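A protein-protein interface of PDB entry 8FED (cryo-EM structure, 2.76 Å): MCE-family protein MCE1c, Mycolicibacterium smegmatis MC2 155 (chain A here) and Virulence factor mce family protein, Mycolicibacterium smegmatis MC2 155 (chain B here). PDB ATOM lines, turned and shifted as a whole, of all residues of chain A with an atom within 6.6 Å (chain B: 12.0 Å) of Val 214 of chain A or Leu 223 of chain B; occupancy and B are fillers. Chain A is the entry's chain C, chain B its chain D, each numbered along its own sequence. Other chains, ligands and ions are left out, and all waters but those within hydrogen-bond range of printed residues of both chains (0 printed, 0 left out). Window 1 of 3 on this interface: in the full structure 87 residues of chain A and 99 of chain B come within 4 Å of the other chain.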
ATOM      1  N   LEU A 207       1.121 -14.656  -5.813  1.00  0.00           N
ATOM      2  CA  LEU A 207       1.607 -15.641  -4.848  1.00  0.00           C
ATOM      3  C   LEU A 207       0.466 -16.223  -4.019  1.00  0.00           C
ATOM      4  O   LEU A 207       0.382 -17.441  -3.825  1.00  0.00           O
ATOM      5  CB  LEU A 207       2.660 -15.014  -3.934  1.00  0.00           C
ATOM      6  CG  LEU A 207       4.064 -14.846  -4.512  1.00  0.00           C
ATOM      7  CD1 LEU A 207       4.985 -14.215  -3.483  1.00  0.00           C
ATOM      8  CD2 LEU A 207       4.611 -16.185  -4.972  1.00  0.00           C
ATOM      9  N   ARG A 210      -1.914 -18.728  -5.632  1.00  0.00           N
ATOM     10  CA  ARG A 210      -1.286 -20.020  -5.886  1.00  0.00           C
ATOM     11  C   ARG A 210      -0.553 -20.558  -4.660  1.00  0.00           C
ATOM     12  O   ARG A 210       0.340 -21.396  -4.801  1.00  0.00           O
ATOM     13  CB  ARG A 210      -0.326 -19.919  -7.071  1.00  0.00           C
ATOM     14  CG  ARG A 210      -0.942 -19.316  -8.319  1.00  0.00           C
ATOM     15  CD  ARG A 210      -2.165 -20.096  -8.757  1.00  0.00           C
ATOM     16  NE  ARG A 210      -2.725 -19.577  -9.999  1.00  0.00           N
ATOM     17  CZ  ARG A 210      -3.776 -20.094 -10.619  1.00  0.00           C
ATOM     18  NH1 ARG A 210      -4.410 -21.153 -10.140  1.00  0.00           N
ATOM     19  NH2 ARG A 210      -4.201 -19.538 -11.750  1.00  0.00           N
ATOM     20  N   SER A 211      -0.911 -20.088  -3.463  1.00  0.00           N
ATOM     21  CA  SER A 211      -0.190 -20.489  -2.256  1.00  0.00           C
ATOM     22  C   SER A 211      -0.351 -21.976  -1.964  1.00  0.00           C
ATOM     23  O   SER A 211       0.607 -22.636  -1.542  1.00  0.00           O
ATOM     24  CB  SER A 211      -0.661 -19.668  -1.063  1.00  0.00           C
ATOM     25  OG  SER A 211       0.013 -20.091   0.104  1.00  0.00           O
ATOM     26  N   THR A 212      -1.558 -22.514  -2.151  1.00  0.00           N
ATOM     27  CA  THR A 212      -1.763 -23.946  -1.961  1.00  0.00           C
ATOM     28  C   THR A 212      -0.893 -24.744  -2.922  1.00  0.00           C
ATOM     29  O   THR A 212      -0.275 -25.744  -2.533  1.00  0.00           O
ATOM     30  CB  THR A 212      -3.240 -24.296  -2.155  1.00  0.00           C
ATOM     31  OG1 THR A 212      -4.026 -23.612  -1.171  1.00  0.00           O
ATOM     32  CG2 THR A 212      -3.462 -25.793  -2.017  1.00  0.00           C
ATOM     33  N   GLN A 213      -0.819 -24.298  -4.177  1.00  0.00           N
ATOM     34  CA  GLN A 213       0.041 -24.952  -5.155  1.00  0.00           C
ATOM     35  C   GLN A 213       1.506 -24.862  -4.746  1.00  0.00           C
ATOM     36  O   GLN A 213       2.257 -25.825  -4.911  1.00  0.00           O
ATOM     37  CB  GLN A 213      -0.169 -24.341  -6.540  1.00  0.00           C
ATOM     38  CG  GLN A 213      -1.480 -24.725  -7.217  1.00  0.00           C
ATOM     39  CD  GLN A 213      -2.686 -24.002  -6.647  1.00  0.00           C
ATOM     40  OE1 GLN A 213      -2.558 -23.142  -5.775  1.00  0.00           O
ATOM     41  NE2 GLN A 213      -3.867 -24.348  -7.143  1.00  0.00           N
ATOM     42  N   VAL A 214       1.932 -23.714  -4.213  1.00  0.00           N
ATOM     43  CA  VAL A 214       3.323 -23.557  -3.788  1.00  0.00           C
ATOM     44  C   VAL A 214       3.649 -24.522  -2.652  1.00  0.00           C
ATOM     45  O   VAL A 214       4.688 -25.196  -2.665  1.00  0.00           O
ATOM     46  CB  VAL A 214       3.602 -22.098  -3.388  1.00  0.00           C
ATOM     47  CG1 VAL A 214       4.938 -21.984  -2.677  1.00  0.00           C
ATOM     48  CG2 VAL A 214       3.586 -21.204  -4.614  1.00  0.00           C
ATOM     49  N   ASN A 215       2.769 -24.599  -1.650  1.00  0.00           N
ATOM     50  CA  ASN A 215       3.012 -25.490  -0.518  1.00  0.00           C
ATOM     51  C   ASN A 215       3.038 -26.949  -0.959  1.00  0.00           C
ATOM     52  O   ASN A 215       3.919 -27.719  -0.548  1.00  0.00           O
ATOM     53  CB  ASN A 215       1.946 -25.275   0.556  1.00  0.00           C
ATOM     54  CG  ASN A 215       2.210 -26.083   1.809  1.00  0.00           C
ATOM     55  OD1 ASN A 215       3.349 -26.448   2.098  1.00  0.00           O
ATOM     56  ND2 ASN A 215       1.155 -26.363   2.563  1.00  0.00           N
ATOM     57  N   GLN A 216       2.076 -27.343  -1.797  1.00  0.00           N
ATOM     58  CA  GLN A 216       2.036 -28.712  -2.295  1.00  0.00           C
ATOM     59  C   GLN A 216       3.272 -29.023  -3.130  1.00  0.00           C
ATOM     60  O   GLN A 216       3.839 -30.115  -3.027  1.00  0.00           O
ATOM     61  CB  GLN A 216       0.758 -28.928  -3.104  1.00  0.00           C
ATOM     62  CG  GLN A 216       0.440 -30.374  -3.410  1.00  0.00           C
ATOM     63  CD  GLN A 216      -0.948 -30.547  -3.990  1.00  0.00           C
ATOM     64  OE1 GLN A 216      -1.640 -29.569  -4.273  1.00  0.00           O
ATOM     65  NE2 GLN A 216      -1.364 -31.794  -4.171  1.00  0.00           N
ATOM     66  N   LEU A 217       3.707 -28.064  -3.951  1.00  0.00           N
ATOM     67  CA  LEU A 217       4.915 -28.229  -4.750  1.00  0.00           C
ATOM     68  C   LEU A 217       6.125 -28.465  -3.859  1.00  0.00           C
ATOM     69  O   LEU A 217       6.922 -29.372  -4.110  1.00  0.00           O
ATOM     70  CB  LEU A 217       5.114 -26.984  -5.621  1.00  0.00           C
ATOM     71  CG  LEU A 217       6.048 -26.901  -6.834  1.00  0.00           C
ATOM     72  CD1 LEU A 217       5.785 -25.584  -7.537  1.00  0.00           C
ATOM     73  CD2 LEU A 217       7.526 -27.008  -6.486  1.00  0.00           C
ATOM     74  N   LEU A 218       6.278 -27.652  -2.813  1.00  0.00           N
ATOM     75  CA  LEU A 218       7.444 -27.787  -1.945  1.00  0.00           C
ATOM     76  C   LEU A 218       7.443 -29.121  -1.207  1.00  0.00           C
ATOM     77  O   LEU A 218       8.481 -29.791  -1.130  1.00  0.00           O
ATOM     78  CB  LEU A 218       7.513 -26.619  -0.963  1.00  0.00           C
ATOM     79  CG  LEU A 218       7.803 -25.260  -1.603  1.00  0.00           C
ATOM     80  CD1 LEU A 218       8.060 -24.199  -0.550  1.00  0.00           C
ATOM     81  CD2 LEU A 218       8.982 -25.365  -2.551  1.00  0.00           C
ATOM     82  N   VAL A 219       6.291 -29.534  -0.668  1.00  0.00           N
ATOM     83  CA  VAL A 219       6.272 -30.783   0.092  1.00  0.00           C
ATOM     84  C   VAL A 219       6.462 -31.985  -0.833  1.00  0.00           C
ATOM     85  O   VAL A 219       7.178 -32.937  -0.492  1.00  0.00           O
ATOM     86  CB  VAL A 219       4.994 -30.893   0.950  1.00  0.00           C
ATOM     87  CG1 VAL A 219       4.934 -29.745   1.947  1.00  0.00           C
ATOM     88  CG2 VAL A 219       3.736 -30.925   0.101  1.00  0.00           C
ATOM     89  N   LYS B 214      -3.147  -8.950   2.970  1.00  0.00           N
ATOM     90  CA  LYS B 214      -4.062 -10.089   2.895  1.00  0.00           C
ATOM     91  C   LYS B 214      -3.468 -11.241   2.089  1.00  0.00           C
ATOM     92  O   LYS B 214      -3.566 -12.408   2.492  1.00  0.00           O
ATOM     93  CB  LYS B 214      -5.398  -9.654   2.295  1.00  0.00           C
ATOM     94  CG  LYS B 214      -6.150  -8.622   3.122  1.00  0.00           C
ATOM     95  CD  LYS B 214      -7.458  -8.195   2.463  1.00  0.00           C
ATOM     96  CE  LYS B 214      -8.614  -9.136   2.785  1.00  0.00           C
ATOM     97  NZ  LYS B 214      -8.507 -10.479   2.151  1.00  0.00           N
ATOM     98  N   SER B 215      -2.851 -10.936   0.944  1.00  0.00           N
ATOM     99  CA  SER B 215      -2.295 -11.993   0.104  1.00  0.00           C
ATOM    100  C   SER B 215      -1.130 -12.697   0.787  1.00  0.00           C
ATOM    101  O   SER B 215      -1.026 -13.930   0.741  1.00  0.00           O
ATOM    102  CB  SER B 215      -1.866 -11.412  -1.239  1.00  0.00           C
ATOM    103  OG  SER B 215      -2.969 -10.835  -1.916  1.00  0.00           O
ATOM    104  N   LEU B 216      -0.241 -11.934   1.426  1.00  0.00           N
ATOM    105  CA  LEU B 216       0.844 -12.545   2.180  1.00  0.00           C
ATOM    106  C   LEU B 216       0.319 -13.329   3.371  1.00  0.00           C
ATOM    107  O   LEU B 216       0.914 -14.340   3.747  1.00  0.00           O
ATOM    108  CB  LEU B 216       1.840 -11.485   2.640  1.00  0.00           C
ATOM    109  CG  LEU B 216       2.683 -10.836   1.544  1.00  0.00           C
ATOM    110  CD1 LEU B 216       3.672  -9.857   2.151  1.00  0.00           C
ATOM    111  CD2 LEU B 216       3.399 -11.897   0.729  1.00  0.00           C
ATOM    112  N   ALA B 217      -0.784 -12.885   3.978  1.00  0.00           N
ATOM    113  CA  ALA B 217      -1.389 -13.663   5.050  1.00  0.00           C
ATOM    114  C   ALA B 217      -1.856 -15.016   4.542  1.00  0.00           C
ATOM    115  O   ALA B 217      -1.617 -16.040   5.186  1.00  0.00           O
ATOM    116  CB  ALA B 217      -2.550 -12.895   5.669  1.00  0.00           C
ATOM    117  N   LEU B 218      -2.516 -15.038   3.383  1.00  0.00           N
ATOM    118  CA  LEU B 218      -2.919 -16.311   2.789  1.00  0.00           C
ATOM    119  C   LEU B 218      -1.706 -17.191   2.507  1.00  0.00           C
ATOM    120  O   LEU B 218      -1.692 -18.385   2.841  1.00  0.00           O
ATOM    121  CB  LEU B 218      -3.716 -16.071   1.506  1.00  0.00           C
ATOM    122  CG  LEU B 218      -5.242 -16.028   1.595  1.00  0.00           C
ATOM    123  CD1 LEU B 218      -5.726 -14.835   2.405  1.00  0.00           C
ATOM    124  CD2 LEU B 218      -5.848 -16.015   0.200  1.00  0.00           C
ATOM    125  N   PHE B 219      -0.666 -16.604   1.907  1.00  0.00           N
ATOM    126  CA  PHE B 219       0.537 -17.358   1.557  1.00  0.00           C
ATOM    127  C   PHE B 219       1.187 -17.974   2.791  1.00  0.00           C
ATOM    128  O   PHE B 219       1.473 -19.179   2.828  1.00  0.00           O
ATOM    129  CB  PHE B 219       1.516 -16.437   0.826  1.00  0.00           C
ATOM    130  CG  PHE B 219       2.800 -17.099   0.422  1.00  0.00           C
ATOM    131  CD1 PHE B 219       2.851 -17.919  -0.692  1.00  0.00           C
ATOM    132  CD2 PHE B 219       3.965 -16.875   1.136  1.00  0.00           C
ATOM    133  CE1 PHE B 219       4.034 -18.520  -1.072  1.00  0.00           C
ATOM    134  CE2 PHE B 219       5.149 -17.473   0.759  1.00  0.00           C
ATOM    135  CZ  PHE B 219       5.184 -18.296  -0.346  1.00  0.00           C
ATOM    136  N   VAL B 220       1.411 -17.162   3.822  1.00  0.00           N
ATOM    137  CA  VAL B 220       2.101 -17.637   5.013  1.00  0.00           C
ATOM    138  C   VAL B 220       1.229 -18.620   5.788  1.00  0.00           C
ATOM    139  O   VAL B 220       1.728 -19.616   6.322  1.00  0.00           O
ATOM    140  CB  VAL B 220       2.545 -16.442   5.875  1.00  0.00           C
ATOM    141  CG1 VAL B 220       3.265 -16.922   7.086  1.00  0.00           C
ATOM    142  CG2 VAL B 220       3.476 -15.547   5.080  1.00  0.00           C
ATOM    143  N   ASN B 221      -0.082 -18.372   5.856  1.00  0.00           N
ATOM    144  CA  ASN B 221      -0.965 -19.297   6.557  1.00  0.00           C
ATOM    145  C   ASN B 221      -1.047 -20.641   5.852  1.00  0.00           C
ATOM    146  O   ASN B 221      -1.296 -21.663   6.501  1.00  0.00           O
ATOM    147  CB  ASN B 221      -2.365 -18.700   6.699  1.00  0.00           C
ATOM    148  CG  ASN B 221      -2.435 -17.618   7.754  1.00  0.00           C
ATOM    149  OD1 ASN B 221      -1.592 -17.549   8.648  1.00  0.00           O
ATOM    150  ND2 ASN B 221      -3.453 -16.773   7.663  1.00  0.00           N
ATOM    151  N   ALA B 222      -0.850 -20.672   4.535  1.00  0.00           N
ATOM    152  CA  ALA B 222      -0.854 -21.954   3.849  1.00  0.00           C
ATOM    153  C   ALA B 222       0.515 -22.617   3.801  1.00  0.00           C
ATOM    154  O   ALA B 222       0.589 -23.822   3.534  1.00  0.00           O
ATOM    155  CB  ALA B 222      -1.388 -21.792   2.424  1.00  0.00           C
ATOM    156  N   LEU B 223       1.599 -21.877   4.049  1.00  0.00           N
ATOM    157  CA  LEU B 223       2.930 -22.470   3.977  1.00  0.00           C
ATOM    158  C   LEU B 223       3.628 -22.660   5.320  1.00  0.00           C
ATOM    159  O   LEU B 223       4.696 -23.281   5.350  1.00  0.00           O
ATOM    160  CB  LEU B 223       3.843 -21.628   3.073  1.00  0.00           C
ATOM    161  CG  LEU B 223       4.063 -22.133   1.648  1.00  0.00           C
ATOM    162  CD1 LEU B 223       2.886 -21.767   0.760  1.00  0.00           C
ATOM    163  CD2 LEU B 223       5.364 -21.593   1.082  1.00  0.00           C
ATOM    164  N   HIS B 224       3.078 -22.153   6.425  1.00  0.00           N
ATOM    165  CA  HIS B 224       3.833 -22.151   7.675  1.00  0.00           C
ATOM    166  C   HIS B 224       3.906 -23.512   8.356  1.00  0.00           C
ATOM    167  O   HIS B 224       4.770 -23.706   9.217  1.00  0.00           O
ATOM    168  CB  HIS B 224       3.234 -21.132   8.647  1.00  0.00           C
ATOM    169  CG  HIS B 224       1.973 -21.593   9.309  1.00  0.00           C
ATOM    170  ND1 HIS B 224       1.962 -22.215  10.539  1.00  0.00           N
ATOM    171  CD2 HIS B 224       0.680 -21.519   8.915  1.00  0.00           C
ATOM    172  CE1 HIS B 224       0.718 -22.506  10.872  1.00  0.00           C
ATOM    173  NE2 HIS B 224      -0.080 -22.094   9.904  1.00  0.00           N
ATOM    174  N   ARG B 225       3.028 -24.451   8.004  1.00  0.00           N
ATOM    175  CA  ARG B 225       2.976 -25.715   8.729  1.00  0.00           C
ATOM    176  C   ARG B 225       4.132 -26.648   8.391  1.00  0.00           C
ATOM    177  O   ARG B 225       4.410 -27.570   9.164  1.00  0.00           O
ATOM    178  CB  ARG B 225       1.651 -26.423   8.448  1.00  0.00           C
ATOM    179  CG  ARG B 225       0.459 -25.805   9.154  1.00  0.00           C
ATOM    180  CD  ARG B 225      -0.805 -26.610   8.913  1.00  0.00           C
ATOM    181  NE  ARG B 225      -1.922 -26.115   9.706  1.00  0.00           N
ATOM    182  CZ  ARG B 225      -2.717 -25.119   9.341  1.00  0.00           C
ATOM    183  NH1 ARG B 225      -2.547 -24.487   8.191  1.00  0.00           N
ATOM    184  NH2 ARG B 225      -3.708 -24.749  10.147  1.00  0.00           N
ATOM    185  N   SER B 226       4.811 -26.432   7.267  1.00  0.00           N
ATOM    186  CA  SER B 226       5.844 -27.339   6.776  1.00  0.00           C
ATOM    187  C   SER B 226       7.265 -26.806   6.948  1.00  0.00           C
ATOM    188  O   SER B 226       8.091 -26.950   6.050  1.00  0.00           O
ATOM    189  CB  SER B 226       5.591 -27.676   5.310  1.00  0.00           C
ATOM    190  OG  SER B 226       4.282 -28.184   5.122  1.00  0.00           O
ATOM    191  N   ASP B 227       7.568 -26.155   8.074  1.00  0.00           N
ATOM    192  CA  ASP B 227       8.906 -25.589   8.256  1.00  0.00           C
ATOM    193  C   ASP B 227       9.979 -26.679   8.264  1.00  0.00           C
ATOM    194  O   ASP B 227      11.025 -26.549   7.606  1.00  0.00           O
ATOM    195  CB  ASP B 227       8.958 -24.760   9.539  1.00  0.00           C
ATOM    196  CG  ASP B 227       8.554 -25.550  10.762  1.00  0.00           C
ATOM    197  OD1 ASP B 227       7.664 -26.418  10.640  1.00  0.00           O
ATOM    198  OD2 ASP B 227       9.125 -25.306  11.845  1.00  0.00           O
ATOM    199  N   GLN B 228       9.722 -27.780   8.972  1.00  0.00           N
ATOM    200  CA  GLN B 228      10.694 -28.865   9.003  1.00  0.00           C
ATOM    201  C   GLN B 228      10.766 -29.559   7.652  1.00  0.00           C
ATOM    202  O   GLN B 228      11.841 -30.009   7.237  1.00  0.00           O
ATOM    203  CB  GLN B 228      10.342 -29.860  10.108  1.00  0.00           C
ATOM    204  CG  GLN B 228      10.174 -29.238  11.489  1.00  0.00           C
ATOM    205  CD  GLN B 228      11.468 -28.679  12.057  1.00  0.00           C
ATOM    206  OE1 GLN B 228      12.560 -28.994  11.583  1.00  0.00           O
ATOM    207  NE2 GLN B 228      11.348 -27.846  13.083  1.00  0.00           N
ATOM    208  N   GLN B 229       9.632 -29.677   6.959  1.00  0.00           N
ATOM    209  CA  GLN B 229       9.667 -30.257   5.623  1.00  0.00           C
ATOM    210  C   GLN B 229      10.467 -29.380   4.670  1.00  0.00           C
ATOM    211  O   GLN B 229      11.110 -29.890   3.751  1.00  0.00           O
ATOM    212  CB  GLN B 229       8.247 -30.458   5.097  1.00  0.00           C
ATOM    213  CG  GLN B 229       7.345 -31.235   6.037  1.00  0.00           C
ATOM    214  CD  GLN B 229       6.637 -32.380   5.346  1.00  0.00           C
ATOM    215  OE1 GLN B 229       6.964 -32.734   4.213  1.00  0.00           O
ATOM    216  NE2 GLN B 229       5.657 -32.964   6.024  1.00  0.00           N
ATOM    217  N   PHE B 230      10.447 -28.060   4.879  1.00  0.00           N
ATOM    218  CA  PHE B 230      11.262 -27.153   4.072  1.00  0.00           C
ATOM    219  C   PHE B 230      12.746 -27.345   4.353  1.00  0.00           C
ATOM    220  O   PHE B 230      13.568 -27.330   3.426  1.00  0.00           O
ATOM    221  CB  PHE B 230      10.862 -25.699   4.327  1.00  0.00           C
ATOM    222  CG  PHE B 230       9.469 -25.363   3.883  1.00  0.00           C
ATOM    223  CD1 PHE B 230       8.799 -26.164   2.974  1.00  0.00           C
ATOM    224  CD2 PHE B 230       8.831 -24.237   4.374  1.00  0.00           C
ATOM    225  CE1 PHE B 230       7.520 -25.853   2.570  1.00  0.00           C
ATOM    226  CE2 PHE B 230       7.553 -23.921   3.970  1.00  0.00           C
ATOM    227  CZ  PHE B 230       6.896 -24.730   3.066  1.00  0.00           C
ATOM    228  N   VAL B 231      13.105 -27.519   5.628  1.00  0.00           N
ATOM    229  CA  VAL B 231      14.501 -27.812   5.960  1.00  0.00           C
ATOM    230  C   VAL B 231      14.932 -29.125   5.317  1.00  0.00           C
ATOM    231  O   VAL B 231      16.032 -29.232   4.753  1.00  0.00           O
ATOM    232  CB  VAL B 231      14.694 -27.844   7.487  1.00  0.00           C
ATOM    233  CG1 VAL B 231      16.114 -28.254   7.833  1.00  0.00           C
ATOM    234  CG2 VAL B 231      14.374 -26.494   8.094  1.00  0.00           C
ATOM    235  N   ALA B 232      14.065 -30.137   5.381  1.00  0.00           N
ATOM    236  CA  ALA B 232      14.352 -31.417   4.745  1.00  0.00           C
ATOM    237  C   ALA B 232      14.493 -31.267   3.236  1.00  0.00           C
ATOM    238  O   ALA B 232      15.355 -31.903   2.623  1.00  0.00           O
ATOM    239  CB  ALA B 232      13.259 -32.428   5.084  1.00  0.00           C
ATOM    240  N   LEU B 233      13.647 -30.438   2.621  1.00  0.00           N
ATOM    241  CA  LEU B 233      13.730 -30.198   1.183  1.00  0.00           C
ATOM    242  C   LEU B 233      15.063 -29.570   0.810  1.00  0.00           C
ATOM    243  O   LEU B 233      15.703 -29.983  -0.162  1.00  0.00           O
ATOM    244  CB  LEU B 233      12.579 -29.296   0.737  1.00  0.00           C
ATOM    245  CG  LEU B 233      12.708 -28.662  -0.650  1.00  0.00           C
ATOM    246  CD1 LEU B 233      12.664 -29.717  -1.743  1.00  0.00           C
ATOM    247  CD2 LEU B 233      11.630 -27.616  -0.868  1.00  0.00           C
ATOM    248  N   ASN B 234      15.492 -28.560   1.569  1.00  0.00           N
ATOM    249  CA  ASN B 234      16.765 -27.913   1.266  1.00  0.00           C
ATOM    250  C   ASN B 234      17.931 -28.882   1.426  1.00  0.00           C
ATOM    251  O   ASN B 234      18.832 -28.927   0.579  1.00  0.00           O
ATOM    252  CB  ASN B 234      16.956 -26.682   2.147  1.00  0.00           C
ATOM    253  CG  ASN B 234      16.095 -25.517   1.714  1.00  0.00           C
ATOM    254  OD1 ASN B 234      15.706 -25.418   0.552  1.00  0.00           O
ATOM    255  ND2 ASN B 234      15.803 -24.619   2.645  1.00  0.00           N
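Among the printed residues, pairs that only touch across the chains: Ser 211 of chain A with Leu 218 of chain B (3.6 Å), Ser 211 of chain A with Ala 222 of chain B (3.2 Å), Ser 211 of chain A with Leu 223 of chain B (3.4 Å), Val 214 of chain A with Phe 219 of chain B (3.9 Å), Val 214 of chain A with Leu 223 of chain B (3.8 Å), Asn 215 of chain A with Leu 223 of chain B (3.6 Å), Asn 215 of chain A with Ser 226 of chain B (3.6 Å), Leu 218 of chain A with Phe 230 of chain B (3.6 Å), Leu 218 of chain A with Leu 233 of chain B (3.8 Å) and Val 219 of chain A with Ser 226 of chain B (3.6 Å).
Of the 21 printed residues of chain B, 7 touch a printed residue of chain A. Hydrophobic or aromatic side chains of chain B within 4 Å of the printed part of chain A: Phe 219, Ala 222, Leu 223, Phe 230 and Leu 233. Along chain A the printed residues that touch a printed residue of chain B span positions 211 to 219. Among the printed residues, 12 pairs touch across the chains.
O of Phe 219 of chain B sits close to OG of Ser 211 of chain A, 3.2 Å away. The backbone carbonyl oxygen (O) of Ala 222 of chain B is in hydrogen-bond range of the side-chain amide nitrogen (ND2) of Asn 215 of chain A, at 2.8 Å.
Val 214 of chain A touches just these residues of chain B: Phe 219 (3.9 Å) and Leu 223 (3.8 Å). Printed residues of chain A within 4 Å of Leu 223 of chain B: Ser 211, Val 214 and Asn 215. Of chain B, only Leu 218 (3.6 Å), Phe 219 (3.1 Å), Ala 222 (3.2 Å) and Leu 223 (3.4 Å) come within 4 Å of Ser 211 of chain A. No residue of chain B comes within 4 Å of Gln 213 of chain A. No residue of chain B comes within 4 Å of Leu 217 of chain A. Leu 218 of chain A touches just these residues of chain B: Phe 230 and Leu 233. Printed residues of chain A within 4 Å of Leu 218 of chain B: Ser 211 (3.6 Å). Printed residues of chain A within 4 Å of Phe 230 of chain B: Leu 218 (3.6 Å). The nearest residue of chain B that does not touch Val 214 of chain A is Phe 230 of chain B (6.0 Å). The nearest printed residue of chain A that does not touch Phe 230 of chain B is Asn 215 of chain A (4.1 Å).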
